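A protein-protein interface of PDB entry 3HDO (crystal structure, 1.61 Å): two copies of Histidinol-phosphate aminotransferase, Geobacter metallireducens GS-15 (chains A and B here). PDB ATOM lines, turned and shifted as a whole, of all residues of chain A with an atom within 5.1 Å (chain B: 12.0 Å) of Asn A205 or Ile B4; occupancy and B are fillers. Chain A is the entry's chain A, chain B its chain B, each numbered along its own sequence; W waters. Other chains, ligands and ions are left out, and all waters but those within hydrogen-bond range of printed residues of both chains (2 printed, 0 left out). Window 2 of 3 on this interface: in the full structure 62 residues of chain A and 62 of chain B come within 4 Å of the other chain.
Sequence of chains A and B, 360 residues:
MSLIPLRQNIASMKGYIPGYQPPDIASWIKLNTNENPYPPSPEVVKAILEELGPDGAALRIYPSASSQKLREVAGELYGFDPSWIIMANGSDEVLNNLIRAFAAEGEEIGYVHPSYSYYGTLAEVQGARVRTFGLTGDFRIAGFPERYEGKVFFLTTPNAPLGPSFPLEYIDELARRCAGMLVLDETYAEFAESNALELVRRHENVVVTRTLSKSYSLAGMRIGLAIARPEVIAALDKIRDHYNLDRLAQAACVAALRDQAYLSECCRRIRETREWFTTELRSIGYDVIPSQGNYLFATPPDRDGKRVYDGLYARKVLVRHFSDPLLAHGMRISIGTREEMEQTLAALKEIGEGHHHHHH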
ATOM      1  N   PHE A 102      -1.894 -23.994 -17.940  1.00  0.00           N
ATOM      2  CA  PHE A 102      -3.016 -24.871 -17.609  1.00  0.00           C
ATOM      3  C   PHE A 102      -2.762 -26.311 -17.198  1.00  0.00           C
ATOM      4  O   PHE A 102      -3.598 -26.908 -16.514  1.00  0.00           O
ATOM      5  CB  PHE A 102      -3.992 -24.887 -18.787  1.00  0.00           C
ATOM      6  CG  PHE A 102      -4.642 -23.567 -19.046  1.00  0.00           C
ATOM      7  CD1 PHE A 102      -5.705 -23.141 -18.263  1.00  0.00           C
ATOM      8  CD2 PHE A 102      -4.168 -22.730 -20.052  1.00  0.00           C
ATOM      9  CE1 PHE A 102      -6.290 -21.895 -18.473  1.00  0.00           C
ATOM     10  CE2 PHE A 102      -4.745 -21.486 -20.268  1.00  0.00           C
ATOM     11  CZ  PHE A 102      -5.809 -21.067 -19.476  1.00  0.00           C
ATOM     12  N   LYS A 151      -6.418 -30.950 -19.737  1.00  0.00           N
ATOM     13  CA  LYS A 151      -6.342 -29.518 -19.471  1.00  0.00           C
ATOM     14  C   LYS A 151      -6.233 -28.665 -20.728  1.00  0.00           C
ATOM     15  O   LYS A 151      -6.639 -27.505 -20.727  1.00  0.00           O
ATOM     16  CB  LYS A 151      -5.168 -29.214 -18.536  1.00  0.00           C
ATOM     17  CG  LYS A 151      -5.262 -29.922 -17.195  1.00  0.00           C
ATOM     18  CD  LYS A 151      -6.556 -29.579 -16.479  1.00  0.00           C
ATOM     19  CE  LYS A 151      -6.692 -30.373 -15.189  1.00  0.00           C
ATOM     20  NZ  LYS A 151      -7.990 -30.117 -14.502  1.00  0.00           N
ATOM     21  N   ALA A 175     -15.405 -27.472 -28.479  1.00  0.00           N
ATOM     22  CA  ALA A 175     -15.215 -26.500 -27.406  1.00  0.00           C
ATOM     23  C   ALA A 175     -16.151 -26.814 -26.243  1.00  0.00           C
ATOM     24  O   ALA A 175     -15.764 -26.729 -25.077  1.00  0.00           O
ATOM     25  CB  ALA A 175     -15.468 -25.082 -27.923  1.00  0.00           C
ATOM     26  N   CYS A 178     -14.920 -29.926 -24.296  1.00  0.00           N
ATOM     27  CA  CYS A 178     -13.638 -29.830 -23.600  1.00  0.00           C
ATOM     28  C   CYS A 178     -13.766 -29.178 -22.232  1.00  0.00           C
ATOM     29  O   CYS A 178     -14.213 -28.034 -22.114  1.00  0.00           O
ATOM     30  CB  CYS A 178     -12.624 -29.043 -24.441  1.00  0.00           C
ATOM     31  SG  CYS A 178     -11.908 -29.956 -25.824  1.00  0.00           S
ATOM     32  N   ALA A 179     -13.361 -29.915 -21.201  1.00  0.00           N
ATOM     33  CA  ALA A 179     -13.412 -29.430 -19.828  1.00  0.00           C
ATOM     34  C   ALA A 179     -12.303 -28.413 -19.580  1.00  0.00           C
ATOM     35  O   ALA A 179     -12.388 -27.599 -18.660  1.00  0.00           O
ATOM     36  CB  ALA A 179     -13.270 -30.598 -18.861  1.00  0.00           C
ATOM     37  N   GLY A 180     -11.258 -28.480 -20.398  1.00  0.00           N
ATOM     38  CA  GLY A 180     -10.151 -27.555 -20.264  1.00  0.00           C
ATOM     39  C   GLY A 180     -10.144 -26.571 -21.413  1.00  0.00           C
ATOM     40  O   GLY A 180     -11.202 -26.186 -21.912  1.00  0.00           O
ATOM     41  N   MET A 181      -8.955 -26.164 -21.837  1.00  0.00           N
ATOM     42  CA  MET A 181      -8.828 -25.216 -22.935  1.00  0.00           C
ATOM     43  C   MET A 181      -8.745 -25.935 -24.275  1.00  0.00           C
ATOM     44  O   MET A 181      -8.241 -27.053 -24.359  1.00  0.00           O
ATOM     45  CB  MET A 181      -7.567 -24.359 -22.760  1.00  0.00           C
ATOM     46  CG  MET A 181      -7.476 -23.620 -21.435  1.00  0.00           C
ATOM     47  SD  MET A 181      -8.956 -22.404 -21.182  1.00  0.00           S
ATOM     48  CE  MET A 181      -8.486 -21.131 -22.517  1.00  0.00           C
ATOM     49  N   LEU A 182      -9.269 -25.289 -25.310  1.00  0.00           N
ATOM     50  CA  LEU A 182      -9.221 -25.816 -26.666  1.00  0.00           C
ATOM     51  C   LEU A 182      -8.402 -24.796 -27.438  1.00  0.00           C
ATOM     52  O   LEU A 182      -8.801 -23.636 -27.572  1.00  0.00           O
ATOM     53  CB  LEU A 182     -10.625 -25.931 -27.271  1.00  0.00           C
ATOM     54  CG  LEU A 182     -10.669 -26.334 -28.750  1.00  0.00           C
ATOM     55  CD1 LEU A 182     -10.005 -27.694 -28.949  1.00  0.00           C
ATOM     56  CD2 LEU A 182     -12.119 -26.374 -29.222  1.00  0.00           C
ATOM     57  N   HIS A 203     -17.054 -18.727 -26.913  1.00  0.00           N
ATOM     58  CA  HIS A 203     -16.709 -19.515 -25.739  1.00  0.00           C
ATOM     59  C   HIS A 203     -15.716 -18.775 -24.858  1.00  0.00           C
ATOM     60  O   HIS A 203     -15.299 -17.662 -25.175  1.00  0.00           O
ATOM     61  CB  HIS A 203     -16.130 -20.869 -26.163  1.00  0.00           C
ATOM     62  CG  HIS A 203     -17.057 -21.673 -27.021  1.00  0.00           C
ATOM     63  ND1 HIS A 203     -17.146 -21.500 -28.385  1.00  0.00           N
ATOM     64  CD2 HIS A 203     -17.965 -22.626 -26.701  1.00  0.00           C
ATOM     65  CE1 HIS A 203     -18.070 -22.311 -28.869  1.00  0.00           C
ATOM     66  NE2 HIS A 203     -18.582 -23.004 -27.869  1.00  0.00           N
ATOM     67  N   GLU A 204     -15.352 -19.397 -23.742  1.00  0.00           N
ATOM     68  CA  GLU A 204     -14.399 -18.809 -22.813  1.00  0.00           C
ATOM     69  C   GLU A 204     -13.137 -19.656 -22.780  1.00  0.00           C
ATOM     70  O   GLU A 204     -12.070 -19.191 -22.365  1.00  0.00           O
ATOM     71  CB  GLU A 204     -14.998 -18.758 -21.407  1.00  0.00           C
ATOM     72  CG  GLU A 204     -16.161 -17.805 -21.261  1.00  0.00           C
ATOM     73  CD  GLU A 204     -16.919 -18.026 -19.969  1.00  0.00           C
ATOM     74  OE1 GLU A 204     -17.619 -19.056 -19.863  1.00  0.00           O
ATOM     75  OE2 GLU A 204     -16.807 -17.177 -19.061  1.00  0.00           O
ATOM     76  N   ASN A 205     -13.261 -20.899 -23.236  1.00  0.00           N
ATOM     77  CA  ASN A 205     -12.137 -21.826 -23.213  1.00  0.00           C
ATOM     78  C   ASN A 205     -11.440 -22.023 -24.550  1.00  0.00           C
ATOM     79  O   ASN A 205     -10.691 -22.986 -24.723  1.00  0.00           O
ATOM     80  CB  ASN A 205     -12.599 -23.187 -22.675  1.00  0.00           C
ATOM     81  CG  ASN A 205     -13.564 -23.893 -23.612  1.00  0.00           C
ATOM     82  OD1 ASN A 205     -14.338 -23.254 -24.329  1.00  0.00           O
ATOM     83  ND2 ASN A 205     -13.535 -25.222 -23.598  1.00  0.00           N
ATOM     84  N   VAL A 206     -11.671 -21.109 -25.486  1.00  0.00           N
ATOM     85  CA  VAL A 206     -11.055 -21.211 -26.801  1.00  0.00           C
ATOM     86  C   VAL A 206      -9.962 -20.176 -27.016  1.00  0.00           C
ATOM     87  O   VAL A 206     -10.127 -19.002 -26.689  1.00  0.00           O
ATOM     88  CB  VAL A 206     -12.109 -21.059 -27.925  1.00  0.00           C
ATOM     89  CG1 VAL A 206     -11.420 -20.915 -29.276  1.00  0.00           C
ATOM     90  CG2 VAL A 206     -13.030 -22.272 -27.945  1.00  0.00           C
ATOM     91  N   VAL A 207      -8.841 -20.628 -27.571  1.00  0.00           N
ATOM     92  CA  VAL A 207      -7.711 -19.756 -27.869  1.00  0.00           C
ATOM     93  C   VAL A 207      -7.302 -20.034 -29.313  1.00  0.00           C
ATOM     94  O   VAL A 207      -7.317 -21.179 -29.753  1.00  0.00           O
ATOM     95  CB  VAL A 207      -6.499 -20.066 -26.956  1.00  0.00           C
ATOM     96  CG1 VAL A 207      -5.326 -19.148 -27.308  1.00  0.00           C
ATOM     97  CG2 VAL A 207      -6.892 -19.905 -25.493  1.00  0.00           C
ATOM     98  N   ILE B   4     -11.522 -21.284 -17.856  1.00  0.00           N
ATOM     99  CA  ILE B   4     -11.271 -22.464 -16.984  1.00  0.00           C
ATOM    100  C   ILE B   4     -10.132 -22.168 -16.013  1.00  0.00           C
ATOM    101  O   ILE B   4      -9.386 -21.205 -16.189  1.00  0.00           O
ATOM    102  CB  ILE B   4     -10.908 -23.723 -17.803  1.00  0.00           C
ATOM    103  CG1 ILE B   4      -9.394 -23.908 -17.828  1.00  0.00           C
ATOM    104  CG2 ILE B   4     -11.477 -23.613 -19.214  1.00  0.00           C
ATOM    105  CD1 ILE B   4      -8.983 -25.283 -18.161  1.00  0.00           C
ATOM    106  N   PRO B   5      -9.988 -22.999 -14.973  1.00  0.00           N
ATOM    107  CA  PRO B   5      -8.943 -22.827 -13.963  1.00  0.00           C
ATOM    108  C   PRO B   5      -7.501 -22.963 -14.436  1.00  0.00           C
ATOM    109  O   PRO B   5      -7.138 -23.899 -15.149  1.00  0.00           O
ATOM    110  CB  PRO B   5      -9.293 -23.889 -12.918  1.00  0.00           C
ATOM    111  CG  PRO B   5     -10.766 -24.026 -13.048  1.00  0.00           C
ATOM    112  CD  PRO B   5     -10.946 -24.035 -14.547  1.00  0.00           C
ATOM    113  N   LEU B   6      -6.688 -22.002 -14.024  1.00  0.00           N
ATOM    114  CA  LEU B   6      -5.266 -22.000 -14.326  1.00  0.00           C
ATOM    115  C   LEU B   6      -4.647 -22.820 -13.209  1.00  0.00           C
ATOM    116  O   LEU B   6      -5.319 -23.136 -12.228  1.00  0.00           O
ATOM    117  CB  LEU B   6      -4.706 -20.586 -14.220  1.00  0.00           C
ATOM    118  CG  LEU B   6      -5.118 -19.512 -15.216  1.00  0.00           C
ATOM    119  CD1 LEU B   6      -4.868 -18.141 -14.597  1.00  0.00           C
ATOM    120  CD2 LEU B   6      -4.333 -19.693 -16.507  1.00  0.00           C
ATOM    121  N   ARG B   7      -3.377 -23.178 -13.353  1.00  0.00           N
ATOM    122  CA  ARG B   7      -2.697 -23.889 -12.285  1.00  0.00           C
ATOM    123  C   ARG B   7      -2.731 -22.862 -11.157  1.00  0.00           C
ATOM    124  O   ARG B   7      -2.626 -21.664 -11.419  1.00  0.00           O
ATOM    125  CB  ARG B   7      -1.253 -24.183 -12.680  1.00  0.00           C
ATOM    126  CG  ARG B   7      -1.102 -25.233 -13.760  1.00  0.00           C
ATOM    127  CD  ARG B   7       0.325 -25.239 -14.269  1.00  0.00           C
ATOM    128  NE  ARG B   7       1.284 -25.471 -13.191  1.00  0.00           N
ATOM    129  CZ  ARG B   7       2.569 -25.139 -13.250  1.00  0.00           C
ATOM    130  NH1 ARG B   7       3.056 -24.558 -14.339  1.00  0.00           N
ATOM    131  NH2 ARG B   7       3.370 -25.380 -12.217  1.00  0.00           N
ATOM    132  N   GLN B   8      -2.888 -23.310  -9.915  1.00  0.00           N
ATOM    133  CA  GLN B   8      -2.949 -22.382  -8.789  1.00  0.00           C
ATOM    134  C   GLN B   8      -1.780 -21.401  -8.725  1.00  0.00           C
ATOM    135  O   GLN B   8      -1.985 -20.205  -8.540  1.00  0.00           O
ATOM    136  CB  GLN B   8      -3.040 -23.155  -7.469  1.00  0.00           C
ATOM    137  CG  GLN B   8      -2.908 -22.283  -6.216  1.00  0.00           C
ATOM    138  CD  GLN B   8      -3.997 -21.229  -6.097  1.00  0.00           C
ATOM    139  OE1 GLN B   8      -4.155 -20.375  -6.970  1.00  0.00           O
ATOM    140  NE2 GLN B   8      -4.752 -21.281  -5.004  1.00  0.00           N
ATOM    141  N   ASN B   9      -0.560 -21.903  -8.884  1.00  0.00           N
ATOM    142  CA  ASN B   9       0.622 -21.048  -8.823  1.00  0.00           C
ATOM    143  C   ASN B   9       0.605 -19.962  -9.894  1.00  0.00           C
ATOM    144  O   ASN B   9       1.058 -18.842  -9.664  1.00  0.00           O
ATOM    145  CB  ASN B   9       1.897 -21.889  -8.956  1.00  0.00           C
ATOM    146  CG  ASN B   9       2.000 -22.587 -10.298  1.00  0.00           C
ATOM    147  OD1 ASN B   9       1.138 -23.386 -10.663  1.00  0.00           O
ATOM    148  ND2 ASN B   9       3.062 -22.284 -11.044  1.00  0.00           N
ATOM    149  N   ILE B  10       0.082 -20.293 -11.068  1.00  0.00           N
ATOM    150  CA  ILE B  10       0.014 -19.326 -12.153  1.00  0.00           C
ATOM    151  C   ILE B  10      -1.015 -18.241 -11.836  1.00  0.00           C
ATOM    152  O   ILE B  10      -0.810 -17.066 -12.140  1.00  0.00           O
ATOM    153  CB  ILE B  10      -0.334 -20.030 -13.485  1.00  0.00           C
ATOM    154  CG1 ILE B  10       0.780 -21.024 -13.841  1.00  0.00           C
ATOM    155  CG2 ILE B  10      -0.515 -19.007 -14.597  1.00  0.00           C
ATOM    156  CD1 ILE B  10       2.157 -20.376 -14.044  1.00  0.00           C
ATOM    157  N   ALA B  11      -2.117 -18.634 -11.206  1.00  0.00           N
ATOM    158  CA  ALA B  11      -3.159 -17.678 -10.851  1.00  0.00           C
ATOM    159  C   ALA B  11      -2.686 -16.741  -9.742  1.00  0.00           C
ATOM    160  O   ALA B  11      -2.915 -15.532  -9.797  1.00  0.00           O
ATOM    161  CB  ALA B  11      -4.420 -18.422 -10.402  1.00  0.00           C
ATOM    162  N   SER B  12      -2.008 -17.310  -8.750  1.00  0.00           N
ATOM    163  CA  SER B  12      -1.511 -16.563  -7.594  1.00  0.00           C
ATOM    164  C   SER B  12      -0.304 -15.662  -7.828  1.00  0.00           C
ATOM    165  O   SER B  12      -0.213 -14.578  -7.249  1.00  0.00           O
ATOM    166  CB  SER B  12      -1.170 -17.534  -6.460  1.00  0.00           C
ATOM    167  OG  SER B  12      -2.333 -18.173  -5.963  1.00  0.00           O
HETATM  168  O   HOH W   1      -6.290 -26.357 -16.041  1.00  0.00           O
HETATM  169  O   HOH W   2     -10.782 -19.617 -19.811  1.00  0.00           O
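The backbone carbonyl oxygen (O) of Gly A180 lies within hydrogen-bond range of the side-chain amide nitrogen (ND2) of Asn A205 (3.0 Å). The backbone carbonyl oxygen (O) of Ala A175 is in hydrogen-bond range of the side-chain amide nitrogen (ND2) of Asn A205, at 3.1 Å. O of Lys A151 is in hydrogen-bond range of N of Met A181, at 2.9 Å. The guanidinium group (NE) of Arg B7 sits close to the side-chain amide oxygen (OD1) of Asn B9 (3.3 Å). The side-chain amide nitrogen of Asn A205 is in hydrogen-bond range of the backbone carbonyl oxygen of Cys A178, 3.3 Å away. The backbone NH of Leu A182 is in hydrogen-bond range of the backbone carbonyl oxygen of Asn A205.
Among the printed residues, pairs that only touch across the chains: Gly A180 with Ile B4 (3.3 Å), Met A181 with Ile B4 (3.4 Å), Phe A102 with Pro B5 (3.5 Å), Phe A102 with Leu B6 (3.5 Å), Asn A205 with Ile B4 (3.7 Å), Phe A102 with Ile B4 (3.8 Å) and Phe A102 with Arg B7 (3.97 Å).
Of chain B, only Ile B4 comes within 4 Å of Asn A205. Ile B4 touches just these residues of chain A: Phe A102, Gly A180, Met A181 and Asn A205. Of the printed residues of chain B, Phe A102 touches Ile B4, Pro B5, Leu B6 and Arg B7. No residue of chain B comes within 4 Å of Lys A151. No residue of chain B comes within 4 Å of Cys A178. No residue of chain B comes within 4 Å of Ala A179. Of the printed residues of chain B, Gly A180 touches Ile B4. Of chain B, only Ile B4 comes within 4 Å of Met A181. Leu A182 touches none of the printed residues of chain B. No residue of chain B comes within 4 Å of His A203. No residue of chain B comes within 4 Å of Glu A204. No residue of chain B comes within 4 Å of Val A206. Printed residues of chain A within 4 Å of Leu B6: Phe A102. Of the printed residues of chain A, Arg B7 touches Phe A102. The nearest printed residue of chain A that does not touch Ile B4 is Lys A151 (4.1 Å).
Of the 13 printed residues of chain A, 4 touch a printed residue of chain B. Hydrophobic or aromatic side chains of chain A that line the printed part of chain B: Phe A102 and Met A181.
No position is printed for both chains.
Water W2 lies within hydrogen-bond range of the backbone NH of Ile B4 (2.7 Å), the backbone carbonyl oxygen of Glu A204 (2.9 Å) and the side-chain sulfur of Met A181 (3.6 Å). Water W1 lies within hydrogen-bond range of the backbone carbonyl oxygen of Pro B5 (2.7 Å) and the backbone carbonyl oxygen of Phe A102 (2.8 Å).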
